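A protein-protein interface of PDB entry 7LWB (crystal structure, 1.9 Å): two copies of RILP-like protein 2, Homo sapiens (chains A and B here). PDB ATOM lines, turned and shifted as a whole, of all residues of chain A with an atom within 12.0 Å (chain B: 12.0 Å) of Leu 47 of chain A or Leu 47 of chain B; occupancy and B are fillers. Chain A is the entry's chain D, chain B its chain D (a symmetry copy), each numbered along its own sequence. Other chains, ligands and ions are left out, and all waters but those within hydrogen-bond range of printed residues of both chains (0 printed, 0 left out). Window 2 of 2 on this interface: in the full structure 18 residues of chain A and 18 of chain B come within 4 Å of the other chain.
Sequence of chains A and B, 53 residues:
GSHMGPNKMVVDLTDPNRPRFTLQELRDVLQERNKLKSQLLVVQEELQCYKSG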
ATOM      1  N   SER A  38      -9.797 -11.209  30.252  1.00  0.00           N
ATOM      2  CA  SER A  38     -10.042  -9.799  30.502  1.00  0.00           C
ATOM      3  C   SER A  38      -8.728  -9.021  30.691  1.00  0.00           C
ATOM      4  O   SER A  38      -8.524  -7.968  30.070  1.00  0.00           O
ATOM      5  CB  SER A  38     -10.943  -9.694  31.736  1.00  0.00           C
ATOM      6  OG  SER A  38     -11.370  -8.364  31.957  1.00  0.00           O
ATOM      7  N   GLN A  39      -7.814  -9.549  31.525  1.00  0.00           N
ATOM      8  CA  GLN A  39      -6.547  -8.856  31.786  1.00  0.00           C
ATOM      9  C   GLN A  39      -5.685  -8.830  30.534  1.00  0.00           C
ATOM     10  O   GLN A  39      -5.023  -7.827  30.252  1.00  0.00           O
ATOM     11  CB  GLN A  39      -5.780  -9.528  32.947  1.00  0.00           C
ATOM     12  CG  GLN A  39      -6.475  -9.450  34.303  1.00  0.00           C
ATOM     13  CD  GLN A  39      -5.963 -10.471  35.375  1.00  0.00           C
ATOM     14  OE1 GLN A  39      -6.187 -10.273  36.579  1.00  0.00           O
ATOM     15  NE2 GLN A  39      -5.308 -11.552  34.937  1.00  0.00           N
ATOM     16  N   LEU A  40      -5.685  -9.923  29.770  1.00  0.00           N
ATOM     17  CA  LEU A  40      -4.892  -9.970  28.547  1.00  0.00           C
ATOM     18  C   LEU A  40      -5.369  -8.934  27.520  1.00  0.00           C
ATOM     19  O   LEU A  40      -4.553  -8.253  26.881  1.00  0.00           O
ATOM     20  CB  LEU A  40      -4.941 -11.377  27.959  1.00  0.00           C
ATOM     21  CG  LEU A  40      -4.352 -11.520  26.558  1.00  0.00           C
ATOM     22  CD1 LEU A  40      -2.838 -11.477  26.659  1.00  0.00           C
ATOM     23  CD2 LEU A  40      -4.853 -12.792  25.816  1.00  0.00           C
ATOM     24  N   LEU A  41      -6.684  -8.790  27.349  1.00  0.00           N
ATOM     25  CA  LEU A  41      -7.178  -7.797  26.393  1.00  0.00           C
ATOM     26  C   LEU A  41      -6.806  -6.393  26.826  1.00  0.00           C
ATOM     27  O   LEU A  41      -6.582  -5.521  25.981  1.00  0.00           O
ATOM     28  CB  LEU A  41      -8.689  -7.905  26.240  1.00  0.00           C
ATOM     29  CG  LEU A  41      -9.145  -9.173  25.537  1.00  0.00           C
ATOM     30  CD1 LEU A  41     -10.628  -9.384  25.802  1.00  0.00           C
ATOM     31  CD2 LEU A  41      -8.844  -9.008  24.041  1.00  0.00           C
ATOM     32  N   VAL A  42      -6.717  -6.163  28.141  1.00  0.00           N
ATOM     33  CA  VAL A  42      -6.350  -4.843  28.645  1.00  0.00           C
ATOM     34  C   VAL A  42      -4.904  -4.520  28.309  1.00  0.00           C
ATOM     35  O   VAL A  42      -4.591  -3.430  27.806  1.00  0.00           O
ATOM     36  CB  VAL A  42      -6.582  -4.757  30.156  1.00  0.00           C
ATOM     37  CG1 VAL A  42      -5.738  -3.600  30.722  1.00  0.00           C
ATOM     38  CG2 VAL A  42      -8.045  -4.576  30.453  1.00  0.00           C
ATOM     39  N   VAL A  43      -3.996  -5.448  28.592  1.00  0.00           N
ATOM     40  CA  VAL A  43      -2.590  -5.162  28.356  1.00  0.00           C
ATOM     41  C   VAL A  43      -2.275  -5.199  26.860  1.00  0.00           C
ATOM     42  O   VAL A  43      -1.306  -4.583  26.404  1.00  0.00           O
ATOM     43  CB  VAL A  43      -1.760  -6.154  29.185  1.00  0.00           C
ATOM     44  CG1 VAL A  43      -0.311  -6.035  28.922  1.00  0.00           C
ATOM     45  CG2 VAL A  43      -2.049  -5.924  30.642  1.00  0.00           C
ATOM     46  N   GLN A  44      -3.093  -5.903  26.069  1.00  0.00           N
ATOM     47  CA  GLN A  44      -2.954  -5.820  24.620  1.00  0.00           C
ATOM     48  C   GLN A  44      -3.383  -4.453  24.116  1.00  0.00           C
ATOM     49  O   GLN A  44      -2.737  -3.870  23.223  1.00  0.00           O
ATOM     50  CB  GLN A  44      -3.783  -6.916  23.955  1.00  0.00           C
ATOM     51  CG  GLN A  44      -3.173  -8.305  24.031  1.00  0.00           C
ATOM     52  CD  GLN A  44      -4.073  -9.361  23.414  1.00  0.00           C
ATOM     53  OE1 GLN A  44      -5.309  -9.243  23.404  1.00  0.00           O
ATOM     54  NE2 GLN A  44      -3.452 -10.404  22.882  1.00  0.00           N
ATOM     55  N   GLU A  45      -4.469  -3.910  24.672  1.00  0.00           N
ATOM     56  CA  GLU A  45      -4.857  -2.566  24.254  1.00  0.00           C
ATOM     57  C   GLU A  45      -3.828  -1.539  24.705  1.00  0.00           C
ATOM     58  O   GLU A  45      -3.578  -0.549  23.998  1.00  0.00           O
ATOM     59  CB  GLU A  45      -6.240  -2.202  24.796  1.00  0.00           C
ATOM     60  CG  GLU A  45      -6.640  -0.799  24.371  1.00  0.00           C
ATOM     61  CD  GLU A  45      -8.047  -0.445  24.777  1.00  0.00           C
ATOM     62  OE1 GLU A  45      -8.664  -1.243  25.542  1.00  0.00           O
ATOM     63  OE2 GLU A  45      -8.509   0.642  24.328  1.00  0.00           O
ATOM     64  N   GLU A  46      -3.208  -1.769  25.867  1.00  0.00           N
ATOM     65  CA  GLU A  46      -2.186  -0.873  26.384  1.00  0.00           C
ATOM     66  C   GLU A  46      -1.025  -0.729  25.406  1.00  0.00           C
ATOM     67  O   GLU A  46      -0.184   0.167  25.575  1.00  0.00           O
ATOM     68  CB  GLU A  46      -1.702  -1.371  27.752  1.00  0.00           C
ATOM     69  CG  GLU A  46      -1.432  -0.240  28.711  1.00  0.00           C
ATOM     70  CD  GLU A  46      -0.821  -0.675  30.040  1.00  0.00           C
ATOM     71  OE1 GLU A  46       0.373  -0.352  30.298  1.00  0.00           O
ATOM     72  OE2 GLU A  46      -1.542  -1.292  30.844  1.00  0.00           O
ATOM     73  N   LEU A  47      -0.997  -1.550  24.351  1.00  0.00           N
ATOM     74  CA  LEU A  47       0.037  -1.481  23.320  1.00  0.00           C
ATOM     75  C   LEU A  47      -0.507  -0.743  22.098  1.00  0.00           C
ATOM     76  O   LEU A  47      -1.008  -1.326  21.134  1.00  0.00           O
ATOM     77  CB  LEU A  47       0.531  -2.882  22.992  1.00  0.00           C
ATOM     78  CG  LEU A  47       1.213  -3.563  24.188  1.00  0.00           C
ATOM     79  CD1 LEU A  47       2.365  -4.447  23.747  1.00  0.00           C
ATOM     80  CD2 LEU A  47       1.696  -2.518  25.143  1.00  0.00           C
ATOM     81  N   GLN A  48      -0.440   0.583  22.188  1.00  0.00           N
ATOM     82  CA  GLN A  48      -0.471   1.486  21.055  1.00  0.00           C
ATOM     83  C   GLN A  48       0.882   2.187  20.870  1.00  0.00           C
ATOM     84  O   GLN A  48       1.037   3.025  19.961  1.00  0.00           O
ATOM     85  CB  GLN A  48      -1.603   2.506  21.245  1.00  0.00           C
ATOM     86  CG  GLN A  48      -1.261   3.624  22.239  1.00  0.00           C
ATOM     87  CD  GLN A  48      -1.170   3.120  23.662  1.00  0.00           C
ATOM     88  OE1 GLN A  48      -2.099   2.481  24.157  1.00  0.00           O
ATOM     89  NE2 GLN A  48      -0.048   3.403  24.328  1.00  0.00           N
ATOM     90  N   CYS A  49       1.859   1.867  21.723  1.00  0.00           N
ATOM     91  CA  CYS A  49       3.243   2.280  21.545  1.00  0.00           C
ATOM     92  C   CYS A  49       3.731   1.759  20.207  1.00  0.00           C
ATOM     93  O   CYS A  49       3.557   0.578  19.908  1.00  0.00           O
ATOM     94  CB  CYS A  49       4.132   1.733  22.670  1.00  0.00           C
ATOM     95  SG  CYS A  49       3.472   1.887  24.369  1.00  0.00           S
ATOM     96  N   SER B  38      -0.331 -17.853  29.886  1.00  0.00           N
ATOM     97  CA  SER B  38       0.913 -17.811  29.139  1.00  0.00           C
ATOM     98  C   SER B  38       1.000 -16.555  28.253  1.00  0.00           C
ATOM     99  O   SER B  38       2.013 -15.842  28.270  1.00  0.00           O
ATOM    100  CB  SER B  38       1.003 -19.094  28.308  1.00  0.00           C
ATOM    101  OG  SER B  38       2.261 -19.218  27.674  1.00  0.00           O
ATOM    102  N   GLN B  39      -0.073 -16.258  27.499  1.00  0.00           N
ATOM    103  CA  GLN B  39      -0.063 -15.096  26.602  1.00  0.00           C
ATOM    104  C   GLN B  39      -0.017 -13.805  27.404  1.00  0.00           C
ATOM    105  O   GLN B  39       0.667 -12.854  27.017  1.00  0.00           O
ATOM    106  CB  GLN B  39      -1.298 -15.104  25.675  1.00  0.00           C
ATOM    107  CG  GLN B  39      -1.352 -16.269  24.690  1.00  0.00           C
ATOM    108  CD  GLN B  39      -2.760 -16.549  24.064  1.00  0.00           C
ATOM    109  OE1 GLN B  39      -2.855 -17.210  23.018  1.00  0.00           O
ATOM    110  NE2 GLN B  39      -3.830 -16.072  24.708  1.00  0.00           N
ATOM    111  N   LEU B  40      -0.737 -13.757  28.526  1.00  0.00           N
ATOM    112  CA  LEU B  40      -0.735 -12.556  29.354  1.00  0.00           C
ATOM    113  C   LEU B  40       0.658 -12.262  29.925  1.00  0.00           C
ATOM    114  O   LEU B  40       1.107 -11.105  29.935  1.00  0.00           O
ATOM    115  CB  LEU B  40      -1.759 -12.707  30.474  1.00  0.00           C
ATOM    116  CG  LEU B  40      -1.706 -11.631  31.557  1.00  0.00           C
ATOM    117  CD1 LEU B  40      -2.310 -10.353  31.003  1.00  0.00           C
ATOM    118  CD2 LEU B  40      -2.385 -12.072  32.885  1.00  0.00           C
ATOM    119  N   LEU B  41       1.365 -13.289  30.399  1.00  0.00           N
ATOM    120  CA  LEU B  41       2.707 -13.050  30.933  1.00  0.00           C
ATOM    121  C   LEU B  41       3.644 -12.555  29.849  1.00  0.00           C
ATOM    122  O   LEU B  41       4.558 -11.774  30.128  1.00  0.00           O
ATOM    123  CB  LEU B  41       3.269 -14.321  31.558  1.00  0.00           C
ATOM    124  CG  LEU B  41       2.564 -14.738  32.837  1.00  0.00           C
ATOM    125  CD1 LEU B  41       2.902 -16.190  33.142  1.00  0.00           C
ATOM    126  CD2 LEU B  41       3.028 -13.792  33.953  1.00  0.00           C
ATOM    127  N   VAL B  42       3.417 -12.984  28.603  1.00  0.00           N
ATOM    128  CA  VAL B  42       4.262 -12.545  27.497  1.00  0.00           C
ATOM    129  C   VAL B  42       4.057 -11.066  27.216  1.00  0.00           C
ATOM    130  O   VAL B  42       5.023 -10.299  27.083  1.00  0.00           O
ATOM    131  CB  VAL B  42       3.982 -13.374  26.240  1.00  0.00           C
ATOM    132  CG1 VAL B  42       4.475 -12.589  25.010  1.00  0.00           C
ATOM    133  CG2 VAL B  42       4.642 -14.721  26.342  1.00  0.00           C
ATOM    134  N   VAL B  43       2.803 -10.640  27.105  1.00  0.00           N
ATOM    135  CA  VAL B  43       2.552  -9.248  26.766  1.00  0.00           C
ATOM    136  C   VAL B  43       2.837  -8.341  27.965  1.00  0.00           C
ATOM    137  O   VAL B  43       3.114  -7.149  27.801  1.00  0.00           O
ATOM    138  CB  VAL B  43       1.113  -9.141  26.240  1.00  0.00           C
ATOM    139  CG1 VAL B  43       0.709  -7.743  25.984  1.00  0.00           C
ATOM    140  CG2 VAL B  43       0.997  -9.959  24.984  1.00  0.00           C
ATOM    141  N   GLN B  44       2.792  -8.890  29.184  1.00  0.00           N
ATOM    142  CA  GLN B  44       3.237  -8.125  30.342  1.00  0.00           C
ATOM    143  C   GLN B  44       4.743  -7.928  30.311  1.00  0.00           C
ATOM    144  O   GLN B  44       5.251  -6.836  30.631  1.00  0.00           O
ATOM    145  CB  GLN B  44       2.821  -8.838  31.627  1.00  0.00           C
ATOM    146  CG  GLN B  44       1.349  -8.699  31.979  1.00  0.00           C
ATOM    147  CD  GLN B  44       0.982  -9.484  33.227  1.00  0.00           C
ATOM    148  OE1 GLN B  44       1.586 -10.518  33.550  1.00  0.00           O
ATOM    149  NE2 GLN B  44      -0.014  -8.985  33.944  1.00  0.00           N
ATOM    150  N   GLU B  45       5.486  -8.969  29.926  1.00  0.00           N
ATOM    151  CA  GLU B  45       6.930  -8.780  29.819  1.00  0.00           C
ATOM    152  C   GLU B  45       7.271  -7.819  28.688  1.00  0.00           C
ATOM    153  O   GLU B  45       8.235  -7.045  28.791  1.00  0.00           O
ATOM    154  CB  GLU B  45       7.643 -10.116  29.610  1.00  0.00           C
ATOM    155  CG  GLU B  45       9.145  -9.919  29.487  1.00  0.00           C
ATOM    156  CD  GLU B  45       9.900 -11.221  29.406  1.00  0.00           C
ATOM    157  OE1 GLU B  45       9.231 -12.289  29.279  1.00  0.00           O
ATOM    158  OE2 GLU B  45      11.160 -11.149  29.458  1.00  0.00           O
ATOM    159  N   GLU B  46       6.477  -7.842  27.612  1.00  0.00           N
ATOM    160  CA  GLU B  46       6.686  -6.949  26.483  1.00  0.00           C
ATOM    161  C   GLU B  46       6.631  -5.487  26.911  1.00  0.00           C
ATOM    162  O   GLU B  46       7.017  -4.601  26.132  1.00  0.00           O
ATOM    163  CB  GLU B  46       5.654  -7.247  25.387  1.00  0.00           C
ATOM    164  CG  GLU B  46       6.240  -7.135  24.003  1.00  0.00           C
ATOM    165  CD  GLU B  46       5.223  -7.290  22.876  1.00  0.00           C
ATOM    166  OE1 GLU B  46       4.944  -6.285  22.163  1.00  0.00           O
ATOM    167  OE2 GLU B  46       4.742  -8.418  22.669  1.00  0.00           O
ATOM    168  N   LEU B  47       6.222  -5.220  28.155  1.00  0.00           N
ATOM    169  CA  LEU B  47       6.169  -3.863  28.698  1.00  0.00           C
ATOM    170  C   LEU B  47       7.390  -3.619  29.585  1.00  0.00           C
ATOM    171  O   LEU B  47       7.373  -3.788  30.805  1.00  0.00           O
ATOM    172  CB  LEU B  47       4.854  -3.654  29.435  1.00  0.00           C
ATOM    173  CG  LEU B  47       3.636  -3.753  28.506  1.00  0.00           C
ATOM    174  CD1 LEU B  47       2.536  -2.793  28.921  1.00  0.00           C
ATOM    175  CD2 LEU B  47       4.062  -3.478  27.099  1.00  0.00           C
ATOM    176  N   GLN B  48       8.484  -3.260  28.917  1.00  0.00           N
ATOM    177  CA  GLN B  48       9.614  -2.567  29.505  1.00  0.00           C
ATOM    178  C   GLN B  48       9.728  -1.137  28.959  1.00  0.00           C
ATOM    179  O   GLN B  48      10.661  -0.397  29.328  1.00  0.00           O
ATOM    180  CB  GLN B  48      10.897  -3.367  29.239  1.00  0.00           C
ATOM    181  CG  GLN B  48      11.432  -3.212  27.809  1.00  0.00           C
ATOM    182  CD  GLN B  48      10.537  -3.874  26.785  1.00  0.00           C
ATOM    183  OE1 GLN B  48      10.213  -5.055  26.913  1.00  0.00           O
ATOM    184  NE2 GLN B  48      10.132  -3.117  25.763  1.00  0.00           N
ATOM    185  N   CYS B  49       8.804  -0.740  28.081  1.00  0.00           N
ATOM    186  CA  CYS B  49       8.656   0.640  27.644  1.00  0.00           C
ATOM    187  C   CYS B  49       8.404   1.505  28.865  1.00  0.00           C
ATOM    188  O   CYS B  49       7.541   1.180  29.679  1.00  0.00           O
ATOM    189  CB  CYS B  49       7.489   0.785  26.657  1.00  0.00           C
ATOM    190  SG  CYS B  49       7.386  -0.477  25.337  1.00  0.00           S
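Gln 39 of chain A touches Leu 40 of chain B, and with the chains exchanged Leu 40 of chain A touches Gln 39 of chain B.
Leu 40 of chain B touches its own counterpart, Leu 40 of chain A.
Val 43 of chain B touches its own counterpart, Val 43 of chain A.
Leu 47 of chain A touches its own counterpart, Leu 47 of chain B.
12 positions are printed for both chains.
Of the 7 pairs that touch across the chains among the printed residues, 7 have their exchanged pair printed and touching as well.
OE1 of Gln 48 of chain A lies close to O of Glu 46 of chain A (3.3 Å).
OE1 of Gln 48 of chain B sits close to O of Glu 46 of chain B.
Leu 47 of chain A touches just these residues of chain B: Glu 46 (3.5 Å) and Leu 47 (3.2 Å).
Of chain A, only Glu 46 (3.5 Å) and Leu 47 (3.2 Å) come within 4 Å of Leu 47 of chain B.
Val 43 of chain A touches just one residue of chain B: Val 43 (3.5 Å).
No residue of chain B comes within 4 Å of Glu 45 of chain A.
No residue of chain B comes within 4 Å of Cys 49 of chain A.
Of chain A, only Val 43 comes within 4 Å of Val 43 of chain B.
No residue of chain A comes within 4 Å of Gln 48 of chain B.
No residue of chain A comes within 4 Å of Cys 49 of chain B.
Of the printed residues of chain B, Gln 39 of chain A touches Leu 40 (3.6 Å).
Of the printed residues of chain A, Gln 39 of chain B touches Leu 40 (3.6 Å).
Printed residues of chain B within 4 Å of Leu 40 of chain A: Gln 39 and Leu 40.
Printed residues of chain A within 4 Å of Leu 40 of chain B: Gln 39 (3.6 Å) and Leu 40 (3.6 Å).
Val 42 of chain B touches none of the printed residues of chain A.
Leu 41 of chain B touches none of the printed residues of chain A.
The nearest printed residue of chain A that does not touch Gln 39 of chain B is Gln 44 of chain A (5.9 Å).
Of the 12 printed residues of chain B, 5 touch a printed residue of chain A.
Hydrophobic or aromatic side chains of chain B that line the printed part of chain A: Leu 40, Val 43 and Leu 47.
Of the 12 printed residues of chain A, 5 touch a printed residue of chain B.
Printed residues of chain A that touch a printed residue of chain B: Gln 39, Leu 40, Val 43, Glu 46 and Leu 47.
Hydrophobic or aromatic side chains of chain A within 4 Å of the printed part of chain B: Leu 40, Val 43 and Leu 47.
Among the printed residues, 7 pairs touch across the chains.
Among the printed residues, no Asp or Glu carboxylate lies within 4 Å of a Lys or Arg side-chain nitrogen of the other chain.
Among the printed residues, merely in contact across the chains: Leu 47 of chain A with Leu 47 of chain B, Glu 46 of chain A with Leu 47 of chain B, Leu 47 of chain A with Glu 46 of chain B, Val 43 of chain A with Val 43 of chain B, Leu 40 of chain A with Leu 40 of chain B, Gln 39 of chain A with Leu 40 of chain B and Leu 40 of chain A with Gln 39 of chain B.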
